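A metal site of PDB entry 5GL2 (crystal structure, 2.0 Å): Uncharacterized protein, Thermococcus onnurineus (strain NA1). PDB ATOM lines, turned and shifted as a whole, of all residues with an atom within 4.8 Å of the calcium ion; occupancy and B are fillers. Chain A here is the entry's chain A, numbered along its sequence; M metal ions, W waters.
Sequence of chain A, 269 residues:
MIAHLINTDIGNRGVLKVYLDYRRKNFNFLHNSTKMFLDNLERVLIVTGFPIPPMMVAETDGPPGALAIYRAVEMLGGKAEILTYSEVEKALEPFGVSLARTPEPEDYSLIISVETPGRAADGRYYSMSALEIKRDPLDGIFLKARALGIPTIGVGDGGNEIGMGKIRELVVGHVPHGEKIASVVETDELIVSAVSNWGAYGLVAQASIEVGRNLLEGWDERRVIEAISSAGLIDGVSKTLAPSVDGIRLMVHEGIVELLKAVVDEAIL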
ATOM      1  N   GLU A  59     -22.708 -12.910  22.476  1.00  0.00           N
ATOM      2  CA  GLU A  59     -22.507 -14.004  23.425  1.00  0.00           C
ATOM      3  C   GLU A  59     -23.250 -13.882  24.761  1.00  0.00           C
ATOM      4  O   GLU A  59     -23.859 -12.865  25.060  1.00  0.00           O
ATOM      5  CB  GLU A  59     -21.021 -14.162  23.709  1.00  0.00           C
ATOM      6  CG  GLU A  59     -20.377 -12.875  24.149  1.00  0.00           C
ATOM      7  CD  GLU A  59     -19.293 -13.099  25.174  1.00  0.00           C
ATOM      8  OE1 GLU A  59     -18.369 -12.260  25.257  1.00  0.00           O
ATOM      9  OE2 GLU A  59     -19.370 -14.117  25.895  1.00  0.00           O
ATOM     10  N   ASP A  61     -21.920 -13.782  27.824  1.00  0.00           N
ATOM     11  CA  ASP A  61     -21.320 -12.972  28.864  1.00  0.00           C
ATOM     12  C   ASP A  61     -21.612 -11.520  28.528  1.00  0.00           C
ATOM     13  O   ASP A  61     -21.266 -11.040  27.456  1.00  0.00           O
ATOM     14  CB  ASP A  61     -19.804 -13.148  28.965  1.00  0.00           C
ATOM     15  CG  ASP A  61     -19.264 -12.528  30.234  1.00  0.00           C
ATOM     16  OD1 ASP A  61     -18.054 -12.263  30.318  1.00  0.00           O
ATOM     17  OD2 ASP A  61     -20.055 -12.306  31.162  1.00  0.00           O
ATOM     18  N   GLU A 115     -19.268  -5.905  29.315  1.00  0.00           N
ATOM     19  CA  GLU A 115     -18.757  -6.722  28.223  1.00  0.00           C
ATOM     20  C   GLU A 115     -19.126  -6.181  26.839  1.00  0.00           C
ATOM     21  O   GLU A 115     -19.810  -6.843  26.063  1.00  0.00           O
ATOM     22  CB  GLU A 115     -19.253  -8.166  28.387  1.00  0.00           C
ATOM     23  CG  GLU A 115     -18.651  -9.140  27.405  1.00  0.00           C
ATOM     24  CD  GLU A 115     -17.140  -9.272  27.565  1.00  0.00           C
ATOM     25  OE1 GLU A 115     -16.433  -8.256  27.545  1.00  0.00           O
ATOM     26  OE2 GLU A 115     -16.656 -10.413  27.714  1.00  0.00           O
ATOM     27  N   ASP A 157     -13.685  -8.406  31.517  1.00  0.00           N
ATOM     28  CA  ASP A 157     -12.844  -9.489  32.003  1.00  0.00           C
ATOM     29  C   ASP A 157     -11.801  -9.967  30.979  1.00  0.00           C
ATOM     30  O   ASP A 157     -11.097 -10.938  31.238  1.00  0.00           O
ATOM     31  CB  ASP A 157     -13.727 -10.675  32.421  1.00  0.00           C
ATOM     32  CG  ASP A 157     -14.506 -11.260  31.265  1.00  0.00           C
ATOM     33  OD1 ASP A 157     -15.066 -10.479  30.468  1.00  0.00           O
ATOM     34  OD2 ASP A 157     -14.552 -12.502  31.149  1.00  0.00           O
ATOM     35  N   SER A 196     -17.411 -11.197  32.903  1.00  0.00           N
ATOM     36  CA  SER A 196     -18.094  -9.915  33.002  1.00  0.00           C
ATOM     37  C   SER A 196     -19.384  -9.934  33.795  1.00  0.00           C
ATOM     38  O   SER A 196     -19.661  -9.000  34.548  1.00  0.00           O
ATOM     39  CB  SER A 196     -18.329  -9.306  31.627  1.00  0.00           C
ATOM     40  OG  SER A 196     -17.097  -8.882  31.095  1.00  0.00           O
ATOM     41  N   ASP A 246     -18.380 -18.117  28.683  1.00  0.00           N
ATOM     42  CA  ASP A 246     -16.923 -18.167  28.520  1.00  0.00           C
ATOM     43  C   ASP A 246     -16.319 -19.547  28.767  1.00  0.00           C
ATOM     44  O   ASP A 246     -15.220 -19.668  29.331  1.00  0.00           O
ATOM     45  CB  ASP A 246     -16.246 -17.173  29.462  1.00  0.00           C
ATOM     46  CG  ASP A 246     -16.459 -15.735  29.057  1.00  0.00           C
ATOM     47  OD1 ASP A 246     -17.113 -15.481  28.013  1.00  0.00           O
ATOM     48  OD2 ASP A 246     -15.961 -14.866  29.800  1.00  0.00           O
HETATM   49 CA    CA M   1     -16.000 -12.501  28.952  1.00  0.00          CA
HETATM   50  O   HOH W   1     -16.638 -13.216  26.512  1.00  0.00           O
HETATM   51  O   HOH W   2     -13.499 -12.460  27.896  1.00  0.00           O
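OG of Ser 196 is in hydrogen-bond range of N of Asp 157 (3.5 Å). The side-chain carboxylate (OD2) of Asp 61 sits at hydrogen-bond distance from the backbone NH (N) of Ser 196, at 3.4 Å. OE2 of Glu 59 lies within hydrogen-bond range of N of Asp 61, 3.2 Å away.
Four residues have an atom within 4 Å of the calcium ion: Asp 61, Glu 115, Asp 157 and Asp 246.
The calcium ion is bound by the side-chain carboxylate (OD1) of Asp 61 (2.5 Å), the side-chain carboxylate (OD2) of Asp 246 (2.5 Å), the side-chain carboxylate (OE2) of Glu 115 (2.5 Å), water W1 (2.6 Å), the side-chain carboxylate (OD2) of Asp 157 (2.6 Å), the side-chain carboxylate (OD1) of Asp 157 (2.7 Å) and water W2 (2.7 Å).
Water W1 bridges the side-chain carboxylate of Asp 246 and the side-chain carboxylate of Glu 59.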
